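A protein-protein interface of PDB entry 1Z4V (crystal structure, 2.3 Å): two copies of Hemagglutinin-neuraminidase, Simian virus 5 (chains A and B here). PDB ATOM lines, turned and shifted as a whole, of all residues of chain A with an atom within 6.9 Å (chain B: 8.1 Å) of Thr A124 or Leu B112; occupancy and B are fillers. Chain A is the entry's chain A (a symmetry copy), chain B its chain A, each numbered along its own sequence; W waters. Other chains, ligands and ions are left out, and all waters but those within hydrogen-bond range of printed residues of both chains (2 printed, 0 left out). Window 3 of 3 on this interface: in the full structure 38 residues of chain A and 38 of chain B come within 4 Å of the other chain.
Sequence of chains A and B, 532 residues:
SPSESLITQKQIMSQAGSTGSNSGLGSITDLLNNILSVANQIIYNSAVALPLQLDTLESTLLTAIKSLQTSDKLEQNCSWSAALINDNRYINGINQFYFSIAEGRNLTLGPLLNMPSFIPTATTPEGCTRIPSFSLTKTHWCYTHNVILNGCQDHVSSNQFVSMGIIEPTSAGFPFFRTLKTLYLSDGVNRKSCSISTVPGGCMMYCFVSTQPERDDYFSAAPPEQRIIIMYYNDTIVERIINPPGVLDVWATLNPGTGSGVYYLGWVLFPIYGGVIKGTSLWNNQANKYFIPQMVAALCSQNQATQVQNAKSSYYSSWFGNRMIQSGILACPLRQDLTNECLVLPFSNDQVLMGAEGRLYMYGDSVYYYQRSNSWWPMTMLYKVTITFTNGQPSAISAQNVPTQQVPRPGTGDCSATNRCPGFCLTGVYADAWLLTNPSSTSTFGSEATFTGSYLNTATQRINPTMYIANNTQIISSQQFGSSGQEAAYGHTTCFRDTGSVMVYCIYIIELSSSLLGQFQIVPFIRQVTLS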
ATOM      1  N   THR A 121      -3.426 -22.151  14.256  1.00  0.00           N
ATOM      2  CA  THR A 121      -2.083 -21.998  13.706  1.00  0.00           C
ATOM      3  C   THR A 121      -1.061 -22.836  14.501  1.00  0.00           C
ATOM      4  O   THR A 121      -1.325 -23.230  15.634  1.00  0.00           O
ATOM      5  CB  THR A 121      -1.703 -20.488  13.766  1.00  0.00           C
ATOM      6  OG1 THR A 121      -2.156 -19.844  12.568  1.00  0.00           O
ATOM      7  CG2 THR A 121      -0.240 -20.288  13.929  1.00  0.00           C
ATOM      8  N   ALA A 122       0.092 -23.105  13.895  1.00  0.00           N
ATOM      9  CA  ALA A 122       1.151 -23.852  14.554  1.00  0.00           C
ATOM     10  C   ALA A 122       1.895 -22.859  15.452  1.00  0.00           C
ATOM     11  O   ALA A 122       1.796 -21.653  15.236  1.00  0.00           O
ATOM     12  CB  ALA A 122       2.095 -24.440  13.517  1.00  0.00           C
ATOM     13  N   THR A 123       2.623 -23.348  16.457  1.00  0.00           N
ATOM     14  CA  THR A 123       3.352 -22.449  17.352  1.00  0.00           C
ATOM     15  C   THR A 123       4.870 -22.603  17.285  1.00  0.00           C
ATOM     16  O   THR A 123       5.594 -22.085  18.139  1.00  0.00           O
ATOM     17  CB  THR A 123       2.892 -22.623  18.823  1.00  0.00           C
ATOM     18  OG1 THR A 123       2.959 -24.011  19.190  1.00  0.00           O
ATOM     19  CG2 THR A 123       1.466 -22.121  18.996  1.00  0.00           C
ATOM     20  N   THR A 124       5.347 -23.345  16.296  1.00  0.00           N
ATOM     21  CA  THR A 124       6.781 -23.521  16.085  1.00  0.00           C
ATOM     22  C   THR A 124       7.011 -23.301  14.595  1.00  0.00           C
ATOM     23  O   THR A 124       6.085 -23.419  13.789  1.00  0.00           O
ATOM     24  CB  THR A 124       7.284 -24.937  16.431  1.00  0.00           C
ATOM     25  OG1 THR A 124       6.617 -25.894  15.609  1.00  0.00           O
ATOM     26  CG2 THR A 124       7.043 -25.261  17.891  1.00  0.00           C
ATOM     27  N   PRO A 125       8.247 -22.953  14.211  1.00  0.00           N
ATOM     28  CA  PRO A 125       8.544 -22.730  12.796  1.00  0.00           C
ATOM     29  C   PRO A 125       8.382 -23.995  11.961  1.00  0.00           C
ATOM     30  O   PRO A 125       7.976 -23.934  10.804  1.00  0.00           O
ATOM     31  CB  PRO A 125       9.992 -22.244  12.824  1.00  0.00           C
ATOM     32  CG  PRO A 125      10.076 -21.525  14.126  1.00  0.00           C
ATOM     33  CD  PRO A 125       9.360 -22.482  15.058  1.00  0.00           C
ATOM     34  N   GLU A 126       8.687 -25.144  12.546  1.00  0.00           N
ATOM     35  CA  GLU A 126       8.596 -26.402  11.810  1.00  0.00           C
ATOM     36  C   GLU A 126       7.261 -27.154  11.930  1.00  0.00           C
ATOM     37  O   GLU A 126       7.017 -28.108  11.186  1.00  0.00           O
ATOM     38  CB  GLU A 126       9.737 -27.340  12.230  1.00  0.00           C
ATOM     39  CG  GLU A 126       9.566 -27.961  13.608  1.00  0.00           C
ATOM     40  CD  GLU A 126      10.069 -27.075  14.748  1.00  0.00           C
ATOM     41  OE1 GLU A 126      10.291 -25.857  14.528  1.00  0.00           O
ATOM     42  OE2 GLU A 126      10.231 -27.609  15.871  1.00  0.00           O
ATOM     43  N   GLY A 127       6.403 -26.744  12.864  1.00  0.00           N
ATOM     44  CA  GLY A 127       5.119 -27.409  13.016  1.00  0.00           C
ATOM     45  C   GLY A 127       4.371 -27.472  11.694  1.00  0.00           C
ATOM     46  O   GLY A 127       4.383 -26.512  10.927  1.00  0.00           O
ATOM     47  N   CYS A 128       3.719 -28.597  11.424  1.00  0.00           N
ATOM     48  CA  CYS A 128       2.982 -28.763  10.172  1.00  0.00           C
ATOM     49  C   CYS A 128       1.494 -29.034  10.347  1.00  0.00           C
ATOM     50  O   CYS A 128       1.107 -30.026  10.961  1.00  0.00           O
ATOM     51  CB  CYS A 128       3.562 -29.916   9.346  1.00  0.00           C
ATOM     52  SG  CYS A 128       2.626 -30.224   7.803  1.00  0.00           S
ATOM     53  N   ILE A 148       1.308 -32.330  12.530  1.00  0.00           N
ATOM     54  CA  ILE A 148       2.530 -33.111  12.690  1.00  0.00           C
ATOM     55  C   ILE A 148       3.501 -32.160  13.361  1.00  0.00           C
ATOM     56  O   ILE A 148       3.689 -31.033  12.904  1.00  0.00           O
ATOM     57  CB  ILE A 148       3.097 -33.566  11.338  1.00  0.00           C
ATOM     58  CG1 ILE A 148       2.046 -34.388  10.593  1.00  0.00           C
ATOM     59  CG2 ILE A 148       4.352 -34.425  11.558  1.00  0.00           C
ATOM     60  CD1 ILE A 148       2.394 -34.664   9.152  1.00  0.00           C
ATOM     61  N   LEU A 149       4.115 -32.605  14.453  1.00  0.00           N
ATOM     62  CA  LEU A 149       5.031 -31.751  15.206  1.00  0.00           C
ATOM     63  C   LEU A 149       6.286 -31.254  14.470  1.00  0.00           C
ATOM     64  O   LEU A 149       6.651 -30.085  14.589  1.00  0.00           O
ATOM     65  CB  LEU A 149       5.427 -32.445  16.513  1.00  0.00           C
ATOM     66  CG  LEU A 149       4.257 -32.884  17.407  1.00  0.00           C
ATOM     67  CD1 LEU A 149       4.811 -33.460  18.715  1.00  0.00           C
ATOM     68  CD2 LEU A 149       3.319 -31.701  17.690  1.00  0.00           C
ATOM     69  N   ASN A 150       6.945 -32.119  13.707  1.00  0.00           N
ATOM     70  CA  ASN A 150       8.145 -31.678  13.004  1.00  0.00           C
ATOM     71  C   ASN A 150       8.091 -31.949  11.516  1.00  0.00           C
ATOM     72  O   ASN A 150       8.204 -33.101  11.083  1.00  0.00           O
ATOM     73  CB  ASN A 150       9.394 -32.356  13.580  1.00  0.00           C
ATOM     74  CG  ASN A 150       9.447 -32.282  15.095  1.00  0.00           C
ATOM     75  OD1 ASN A 150       9.028 -33.218  15.787  1.00  0.00           O
ATOM     76  ND2 ASN A 150       9.946 -31.163  15.622  1.00  0.00           N
ATOM     77  N   LEU A 516       6.913 -17.419   8.872  1.00  0.00           N
ATOM     78  CA  LEU A 516       6.991 -17.135  10.298  1.00  0.00           C
ATOM     79  C   LEU A 516       6.709 -18.355  11.168  1.00  0.00           C
ATOM     80  O   LEU A 516       7.638 -18.959  11.705  1.00  0.00           O
ATOM     81  CB  LEU A 516       6.017 -16.003  10.642  1.00  0.00           C
ATOM     82  CG  LEU A 516       6.353 -15.165  11.876  1.00  0.00           C
ATOM     83  CD1 LEU A 516       7.771 -14.626  11.764  1.00  0.00           C
ATOM     84  CD2 LEU A 516       5.357 -14.030  11.996  1.00  0.00           C
ATOM     85  N   LEU A 517       5.434 -18.717  11.311  1.00  0.00           N
ATOM     86  CA  LEU A 517       5.048 -19.871  12.128  1.00  0.00           C
ATOM     87  C   LEU A 517       4.535 -21.051  11.315  1.00  0.00           C
ATOM     88  O   LEU A 517       3.629 -20.905  10.496  1.00  0.00           O
ATOM     89  CB  LEU A 517       3.981 -19.464  13.149  1.00  0.00           C
ATOM     90  CG  LEU A 517       4.447 -18.805  14.456  1.00  0.00           C
ATOM     91  CD1 LEU A 517       5.331 -19.772  15.224  1.00  0.00           C
ATOM     92  CD2 LEU A 517       5.206 -17.532  14.158  1.00  0.00           C
ATOM     93  N   GLY A 518       5.131 -22.221  11.551  1.00  0.00           N
ATOM     94  CA  GLY A 518       4.734 -23.435  10.857  1.00  0.00           C
ATOM     95  C   GLY A 518       5.087 -23.532   9.379  1.00  0.00           C
ATOM     96  O   GLY A 518       5.399 -22.528   8.736  1.00  0.00           O
ATOM     97  N   GLN A 519       5.044 -24.754   8.846  1.00  0.00           N
ATOM     98  CA  GLN A 519       5.321 -25.006   7.431  1.00  0.00           C
ATOM     99  C   GLN A 519       4.205 -24.352   6.616  1.00  0.00           C
ATOM    100  O   GLN A 519       4.446 -23.667   5.631  1.00  0.00           O
ATOM    101  CB  GLN A 519       5.320 -26.508   7.155  1.00  0.00           C
ATOM    102  CG  GLN A 519       6.260 -27.305   8.036  1.00  0.00           C
ATOM    103  CD  GLN A 519       7.701 -27.238   7.554  1.00  0.00           C
ATOM    104  OE1 GLN A 519       8.054 -27.858   6.546  1.00  0.00           O
ATOM    105  NE2 GLN A 519       8.534 -26.477   8.262  1.00  0.00           N
ATOM    106  N   LEU B 109      15.657 -22.437  29.401  1.00  0.00           N
ATOM    107  CA  LEU B 109      14.472 -22.553  28.551  1.00  0.00           C
ATOM    108  C   LEU B 109      14.597 -23.776  27.597  1.00  0.00           C
ATOM    109  O   LEU B 109      15.644 -24.015  27.051  1.00  0.00           O
ATOM    110  CB  LEU B 109      14.324 -21.281  27.700  1.00  0.00           C
ATOM    111  CG  LEU B 109      14.115 -19.975  28.476  1.00  0.00           C
ATOM    112  CD1 LEU B 109      14.320 -18.797  27.551  1.00  0.00           C
ATOM    113  CD2 LEU B 109      12.721 -19.950  29.082  1.00  0.00           C
ATOM    114  N   GLY B 110      13.510 -24.531  27.443  1.00  0.00           N
ATOM    115  CA  GLY B 110      13.567 -25.682  26.543  1.00  0.00           C
ATOM    116  C   GLY B 110      13.164 -25.291  25.121  1.00  0.00           C
ATOM    117  O   GLY B 110      13.025 -24.103  24.861  1.00  0.00           O
ATOM    118  N   PRO B 111      13.065 -26.219  24.163  1.00  0.00           N
ATOM    119  CA  PRO B 111      12.655 -25.812  22.810  1.00  0.00           C
ATOM    120  C   PRO B 111      11.217 -25.354  22.764  1.00  0.00           C
ATOM    121  O   PRO B 111      10.425 -25.678  23.651  1.00  0.00           O
ATOM    122  CB  PRO B 111      12.763 -27.107  21.998  1.00  0.00           C
ATOM    123  CG  PRO B 111      13.802 -27.876  22.654  1.00  0.00           C
ATOM    124  CD  PRO B 111      14.088 -27.270  24.048  1.00  0.00           C
ATOM    125  N   LEU B 112      10.877 -24.625  21.723  1.00  0.00           N
ATOM    126  CA  LEU B 112       9.520 -24.210  21.597  1.00  0.00           C
ATOM    127  C   LEU B 112       8.784 -25.486  21.132  1.00  0.00           C
ATOM    128  O   LEU B 112       9.342 -26.326  20.414  1.00  0.00           O
ATOM    129  CB  LEU B 112       9.423 -23.056  20.553  1.00  0.00           C
ATOM    130  CG  LEU B 112       9.977 -21.724  21.127  1.00  0.00           C
ATOM    131  CD1 LEU B 112      10.097 -20.727  19.994  1.00  0.00           C
ATOM    132  CD2 LEU B 112       9.080 -21.183  22.223  1.00  0.00           C
ATOM    133  N   LEU B 113       7.580 -25.673  21.652  1.00  0.00           N
ATOM    134  CA  LEU B 113       6.806 -26.867  21.339  1.00  0.00           C
ATOM    135  C   LEU B 113       5.599 -26.470  20.492  1.00  0.00           C
ATOM    136  O   LEU B 113       5.050 -25.370  20.643  1.00  0.00           O
ATOM    137  CB  LEU B 113       6.356 -27.523  22.648  1.00  0.00           C
ATOM    138  CG  LEU B 113       7.483 -27.808  23.659  1.00  0.00           C
ATOM    139  CD1 LEU B 113       6.887 -28.241  24.976  1.00  0.00           C
ATOM    140  CD2 LEU B 113       8.416 -28.898  23.122  1.00  0.00           C
ATOM    141  N   ASN B 114       5.207 -27.357  19.585  1.00  0.00           N
ATOM    142  CA  ASN B 114       4.088 -27.069  18.691  1.00  0.00           C
ATOM    143  C   ASN B 114       2.738 -27.595  19.145  1.00  0.00           C
ATOM    144  O   ASN B 114       2.522 -28.797  19.225  1.00  0.00           O
ATOM    145  CB  ASN B 114       4.357 -27.608  17.287  1.00  0.00           C
ATOM    146  CG  ASN B 114       3.253 -27.235  16.302  1.00  0.00           C
ATOM    147  OD1 ASN B 114       3.062 -26.046  16.004  1.00  0.00           O
ATOM    148  ND2 ASN B 114       2.532 -28.201  15.818  1.00  0.00           N
ATOM    149  N   MET B 115       1.828 -26.671  19.422  1.00  0.00           N
ATOM    150  CA  MET B 115       0.478 -27.016  19.825  1.00  0.00           C
ATOM    151  C   MET B 115      -0.464 -26.184  18.965  1.00  0.00           C
ATOM    152  O   MET B 115      -0.056 -25.166  18.409  1.00  0.00           O
ATOM    153  CB  MET B 115       0.251 -26.689  21.307  1.00  0.00           C
ATOM    154  CG  MET B 115       0.344 -25.226  21.630  1.00  0.00           C
ATOM    155  SD  MET B 115      -0.110 -24.857  23.338  1.00  0.00           S
ATOM    156  CE  MET B 115      -0.231 -23.060  23.245  1.00  0.00           C
ATOM    157  N   PHE B 174       3.029 -32.600  26.431  1.00  0.00           N
ATOM    158  CA  PHE B 174       2.796 -31.193  26.718  1.00  0.00           C
ATOM    159  C   PHE B 174       1.342 -30.752  26.551  1.00  0.00           C
ATOM    160  O   PHE B 174       0.536 -31.459  25.971  1.00  0.00           O
ATOM    161  CB  PHE B 174       3.780 -30.295  25.952  1.00  0.00           C
ATOM    162  CG  PHE B 174       3.821 -30.512  24.472  1.00  0.00           C
ATOM    163  CD1 PHE B 174       2.911 -29.864  23.635  1.00  0.00           C
ATOM    164  CD2 PHE B 174       4.830 -31.292  23.905  1.00  0.00           C
ATOM    165  CE1 PHE B 174       3.011 -29.980  22.236  1.00  0.00           C
ATOM    166  CE2 PHE B 174       4.939 -31.420  22.519  1.00  0.00           C
ATOM    167  CZ  PHE B 174       4.033 -30.763  21.683  1.00  0.00           C
ATOM    168  N   MET B 467      12.572 -14.453  24.297  1.00  0.00           N
ATOM    169  CA  MET B 467      12.066 -15.083  25.506  1.00  0.00           C
ATOM    170  C   MET B 467      13.258 -15.330  26.419  1.00  0.00           C
ATOM    171  O   MET B 467      14.350 -15.654  25.941  1.00  0.00           O
ATOM    172  CB  MET B 467      11.340 -16.379  25.150  1.00  0.00           C
ATOM    173  CG  MET B 467       9.994 -16.098  24.457  1.00  0.00           C
ATOM    174  SD  MET B 467       9.213 -17.526  23.687  1.00  0.00           S
ATOM    175  CE  MET B 467       9.491 -17.195  21.992  1.00  0.00           C
ATOM    176  N   GLN B 479      16.422 -16.854  24.245  1.00  0.00           N
ATOM    177  CA  GLN B 479      16.385 -17.299  22.869  1.00  0.00           C
ATOM    178  C   GLN B 479      15.510 -16.353  22.066  1.00  0.00           C
ATOM    179  O   GLN B 479      14.303 -16.211  22.311  1.00  0.00           O
ATOM    180  CB  GLN B 479      15.850 -18.731  22.774  1.00  0.00           C
ATOM    181  CG  GLN B 479      16.011 -19.384  21.386  1.00  0.00           C
ATOM    182  CD  GLN B 479      15.482 -20.814  21.366  1.00  0.00           C
ATOM    183  OE1 GLN B 479      15.020 -21.329  22.385  1.00  0.00           O
ATOM    184  NE2 GLN B 479      15.545 -21.461  20.209  1.00  0.00           N
ATOM    185  N   GLN B 480      16.140 -15.680  21.121  1.00  0.00           N
ATOM    186  CA  GLN B 480      15.453 -14.747  20.256  1.00  0.00           C
ATOM    187  C   GLN B 480      14.604 -15.524  19.268  1.00  0.00           C
ATOM    188  O   GLN B 480      14.975 -16.617  18.857  1.00  0.00           O
ATOM    189  CB  GLN B 480      16.479 -13.911  19.504  1.00  0.00           C
ATOM    190  CG  GLN B 480      15.899 -12.824  18.626  1.00  0.00           C
ATOM    191  CD  GLN B 480      16.982 -11.901  18.104  1.00  0.00           C
ATOM    192  OE1 GLN B 480      17.866 -11.488  18.856  1.00  0.00           O
ATOM    193  NE2 GLN B 480      16.913 -11.562  16.823  1.00  0.00           N
ATOM    194  N   PHE B 481      13.449 -14.975  18.909  1.00  0.00           N
ATOM    195  CA  PHE B 481      12.601 -15.635  17.924  1.00  0.00           C
ATOM    196  C   PHE B 481      12.704 -14.886  16.600  1.00  0.00           C
ATOM    197  O   PHE B 481      12.642 -13.659  16.572  1.00  0.00           O
ATOM    198  CB  PHE B 481      11.132 -15.656  18.346  1.00  0.00           C
ATOM    199  CG  PHE B 481      10.233 -16.215  17.289  1.00  0.00           C
ATOM    200  CD1 PHE B 481      10.185 -17.587  17.056  1.00  0.00           C
ATOM    201  CD2 PHE B 481       9.518 -15.372  16.453  1.00  0.00           C
ATOM    202  CE1 PHE B 481       9.435 -18.109  16.003  1.00  0.00           C
ATOM    203  CE2 PHE B 481       8.771 -15.880  15.405  1.00  0.00           C
ATOM    204  CZ  PHE B 481       8.732 -17.259  15.176  1.00  0.00           C
ATOM    205  N   GLY B 482      12.845 -15.627  15.507  1.00  0.00           N
ATOM    206  CA  GLY B 482      12.945 -14.996  14.200  1.00  0.00           C
ATOM    207  C   GLY B 482      14.314 -14.380  13.968  1.00  0.00           C
ATOM    208  O   GLY B 482      15.215 -14.535  14.785  1.00  0.00           O
ATOM    209  N   CYS B 506       5.661 -22.636  30.240  1.00  0.00           N
ATOM    210  CA  CYS B 506       5.301 -21.226  30.246  1.00  0.00           C
ATOM    211  C   CYS B 506       4.808 -20.902  28.861  1.00  0.00           C
ATOM    212  O   CYS B 506       5.335 -21.401  27.865  1.00  0.00           O
ATOM    213  CB  CYS B 506       6.482 -20.329  30.557  1.00  0.00           C
ATOM    214  SG  CYS B 506       7.188 -20.511  32.214  1.00  0.00           S
ATOM    215  N   ILE B 507       3.774 -20.082  28.805  1.00  0.00           N
ATOM    216  CA  ILE B 507       3.235 -19.666  27.542  1.00  0.00           C
ATOM    217  C   ILE B 507       3.624 -18.196  27.399  1.00  0.00           C
ATOM    218  O   ILE B 507       3.439 -17.401  28.328  1.00  0.00           O
ATOM    219  CB  ILE B 507       1.696 -19.855  27.520  1.00  0.00           C
ATOM    220  CG1 ILE B 507       1.103 -19.239  26.262  1.00  0.00           C
ATOM    221  CG2 ILE B 507       1.067 -19.207  28.734  1.00  0.00           C
ATOM    222  CD1 ILE B 507      -0.409 -19.386  26.191  1.00  0.00           C
ATOM    223  N   TYR B 508       4.206 -17.847  26.258  1.00  0.00           N
ATOM    224  CA  TYR B 508       4.591 -16.471  26.008  1.00  0.00           C
ATOM    225  C   TYR B 508       3.713 -15.955  24.874  1.00  0.00           C
ATOM    226  O   TYR B 508       3.935 -16.294  23.710  1.00  0.00           O
ATOM    227  CB  TYR B 508       6.066 -16.380  25.589  1.00  0.00           C
ATOM    228  CG  TYR B 508       7.010 -17.023  26.569  1.00  0.00           C
ATOM    229  CD1 TYR B 508       7.138 -18.418  26.633  1.00  0.00           C
ATOM    230  CD2 TYR B 508       7.748 -16.249  27.460  1.00  0.00           C
ATOM    231  CE1 TYR B 508       7.965 -19.015  27.556  1.00  0.00           C
ATOM    232  CE2 TYR B 508       8.588 -16.842  28.389  1.00  0.00           C
ATOM    233  CZ  TYR B 508       8.689 -18.228  28.432  1.00  0.00           C
ATOM    234  OH  TYR B 508       9.514 -18.825  29.379  1.00  0.00           O
ATOM    235  N   ILE B 510       2.908 -13.425  22.413  1.00  0.00           N
ATOM    236  CA  ILE B 510       3.601 -12.302  21.796  1.00  0.00           C
ATOM    237  C   ILE B 510       2.962 -11.765  20.524  1.00  0.00           C
ATOM    238  O   ILE B 510       2.617 -12.525  19.627  1.00  0.00           O
ATOM    239  CB  ILE B 510       5.081 -12.706  21.473  1.00  0.00           C
ATOM    240  CG1 ILE B 510       5.804 -13.081  22.768  1.00  0.00           C
ATOM    241  CG2 ILE B 510       5.821 -11.562  20.791  1.00  0.00           C
ATOM    242  CD1 ILE B 510       7.174 -13.675  22.531  1.00  0.00           C
ATOM    243  N   VAL B 523       0.833 -14.779  18.875  1.00  0.00           N
ATOM    244  CA  VAL B 523       1.207 -16.175  19.009  1.00  0.00           C
ATOM    245  C   VAL B 523       1.405 -16.634  20.447  1.00  0.00           C
ATOM    246  O   VAL B 523       2.064 -15.965  21.241  1.00  0.00           O
ATOM    247  CB  VAL B 523       2.518 -16.449  18.233  1.00  0.00           C
ATOM    248  CG1 VAL B 523       2.928 -17.911  18.388  1.00  0.00           C
ATOM    249  CG2 VAL B 523       2.337 -16.091  16.760  1.00  0.00           C
ATOM    250  N   PRO B 524       0.799 -17.775  20.807  1.00  0.00           N
ATOM    251  CA  PRO B 524       0.946 -18.305  22.161  1.00  0.00           C
ATOM    252  C   PRO B 524       2.105 -19.304  22.141  1.00  0.00           C
ATOM    253  O   PRO B 524       1.892 -20.508  22.006  1.00  0.00           O
ATOM    254  CB  PRO B 524      -0.404 -18.975  22.414  1.00  0.00           C
ATOM    255  CG  PRO B 524      -0.740 -19.532  21.074  1.00  0.00           C
ATOM    256  CD  PRO B 524      -0.340 -18.413  20.118  1.00  0.00           C
ATOM    257  N   PHE B 525       3.337 -18.803  22.226  1.00  0.00           N
ATOM    258  CA  PHE B 525       4.503 -19.687  22.228  1.00  0.00           C
ATOM    259  C   PHE B 525       4.472 -20.475  23.529  1.00  0.00           C
ATOM    260  O   PHE B 525       4.043 -19.969  24.562  1.00  0.00           O
ATOM    261  CB  PHE B 525       5.809 -18.882  22.181  1.00  0.00           C
ATOM    262  CG  PHE B 525       6.117 -18.290  20.840  1.00  0.00           C
ATOM    263  CD1 PHE B 525       6.606 -19.081  19.810  1.00  0.00           C
ATOM    264  CD2 PHE B 525       5.910 -16.935  20.609  1.00  0.00           C
ATOM    265  CE1 PHE B 525       6.887 -18.533  18.553  1.00  0.00           C
ATOM    266  CE2 PHE B 525       6.186 -16.369  19.355  1.00  0.00           C
ATOM    267  CZ  PHE B 525       6.673 -17.166  18.325  1.00  0.00           C
ATOM    268  N   ILE B 526       4.926 -21.716  23.482  1.00  0.00           N
ATOM    269  CA  ILE B 526       4.946 -22.515  24.678  1.00  0.00           C
ATOM    270  C   ILE B 526       6.198 -23.373  24.716  1.00  0.00           C
ATOM    271  O   ILE B 526       6.628 -23.914  23.707  1.00  0.00           O
ATOM    272  CB  ILE B 526       3.702 -23.422  24.769  1.00  0.00           C
ATOM    273  CG1 ILE B 526       3.788 -24.276  26.035  1.00  0.00           C
ATOM    274  CG2 ILE B 526       3.609 -24.309  23.549  1.00  0.00           C
ATOM    275  CD1 ILE B 526       2.521 -25.053  26.327  1.00  0.00           C
ATOM    276  N   ARG B 527       6.808 -23.470  25.881  1.00  0.00           N
ATOM    277  CA  ARG B 527       7.984 -24.292  26.035  1.00  0.00           C
ATOM    278  C   ARG B 527       8.112 -24.700  27.500  1.00  0.00           C
ATOM    279  O   ARG B 527       7.260 -24.393  28.306  1.00  0.00           O
ATOM    280  CB  ARG B 527       9.237 -23.546  25.565  1.00  0.00           C
ATOM    281  CG  ARG B 527       9.648 -22.321  26.359  1.00  0.00           C
ATOM    282  CD  ARG B 527      11.031 -21.870  25.871  1.00  0.00           C
ATOM    283  NE  ARG B 527      10.985 -20.772  24.927  1.00  0.00           N
ATOM    284  CZ  ARG B 527      11.834 -20.596  23.918  1.00  0.00           C
ATOM    285  NH1 ARG B 527      12.816 -21.454  23.692  1.00  0.00           N
ATOM    286  NH2 ARG B 527      11.696 -19.538  23.128  1.00  0.00           N
ATOM    287  N   GLN B 528       9.166 -25.425  27.823  1.00  0.00           N
ATOM    288  CA  GLN B 528       9.356 -25.846  29.193  1.00  0.00           C
ATOM    289  C   GLN B 528      10.475 -25.042  29.840  1.00  0.00           C
ATOM    290  O   GLN B 528      11.383 -24.577  29.164  1.00  0.00           O
ATOM    291  CB  GLN B 528       9.705 -27.337  29.234  1.00  0.00           C
ATOM    292  CG  GLN B 528      10.094 -27.821  30.622  1.00  0.00           C
ATOM    293  CD  GLN B 528      10.471 -29.290  30.641  1.00  0.00           C
ATOM    294  OE1 GLN B 528      10.647 -29.917  29.579  1.00  0.00           O
ATOM    295  NE2 GLN B 528      10.601 -29.853  31.848  1.00  0.00           N
HETATM  296  O   HOH W   1      10.936 -26.033  18.277  1.00  0.00           O
HETATM  297  O   HOH W   2       5.918 -22.818  21.066  1.00  0.00           O
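The side-chain hydroxyl of Thr A123 is in hydrogen-bond range of the backbone carbonyl oxygen of Leu B113 (2.9 Å). The side-chain amide oxygen (OD1) of Asn B114 sits at hydrogen-bond distance from the backbone NH (N) of Thr A123, 2.8 Å away. The side-chain hydroxyl (OG1) of Thr A123 sits at hydrogen-bond distance from the backbone NH (N) of Met B115, at 2.9 Å.
N of Leu B113 is in hydrogen-bond range of O of Ile B526 (2.9 Å). N of Tyr B508 sits at hydrogen-bond distance from O of Phe B525 (2.7 Å). OG1 of Thr A124 sits at hydrogen-bond distance from N of Gly A127 (2.9 Å). O of Thr A124 is in hydrogen-bond range of N of Gly A518, 2.7 Å away. O of Pro A125 sits close to N of Gly A518 (3.4 Å). The backbone carbonyl oxygen (O) of Gly A127 sits at hydrogen-bond distance from the backbone NH (N) of Gln A519, 2.8 Å away.
CD1 of Phe B525 touches O of Thr A123 (3.6 Å). O of Leu B112 touches CG2 of Thr A124, 3.6 Å away. C of Leu B113 touches CG2 of Thr A124, 3.2 Å away. Thr A124 touches Asn B114 (CG2 to N, 3.3 Å). Phe B481 touches Pro A125 (CE1 to CG, 3.95 Å). Gly A127 touches Asn B114. CD2 of Leu A149 touches O of Asn B114 (3.4 Å). Phe B481 touches Leu A516. Leu A517 touches Phe B481. Phe B525 touches Leu A517.
Thr A124 touches three residues of chain B. Pro A125 touches just one residue of chain B: Phe B481. Printed residues of chain B within 4 Å of Gly A127: Asn B114 (3.8 Å). Of the printed residues of chain B, Leu A149 touches Asn B114 (3.4 Å). Of chain A, only Thr A124 comes within 4 Å of Leu B112. Ile B507 touches none of the printed residues of chain A. Arg B527 touches none of the printed residues of chain A. The nearest residue of chain B that does not touch Thr A124 is Phe B525 (5.5 Å). The nearest residue of chain A that does not touch Leu B112 is Thr A123 (4.6 Å).
Of the 23 printed residues of chain B, 7 touch a printed residue of chain A. Printed residues of chain B that touch a printed residue of chain A: Leu B112, Leu B113, Asn B114, Met B115, Phe B481, Pro B524 and Phe B525. Hydrophobic or aromatic side chains of chain A that line the printed part of chain B: Ala A122, Pro A125, Leu A149, Leu A516 and Leu A517. Among the printed residues, 16 pairs touch across the chains.
No position is printed for both chains.
Water W1 bridges O of Leu B112 (2.7 Å) and OE2 of Glu A126 (3.0 Å). Water W2 lies within hydrogen-bond range of the backbone carbonyl oxygen of Leu B113, the backbone NH of Ile B526 and the backbone carbonyl oxygen of Thr A123.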
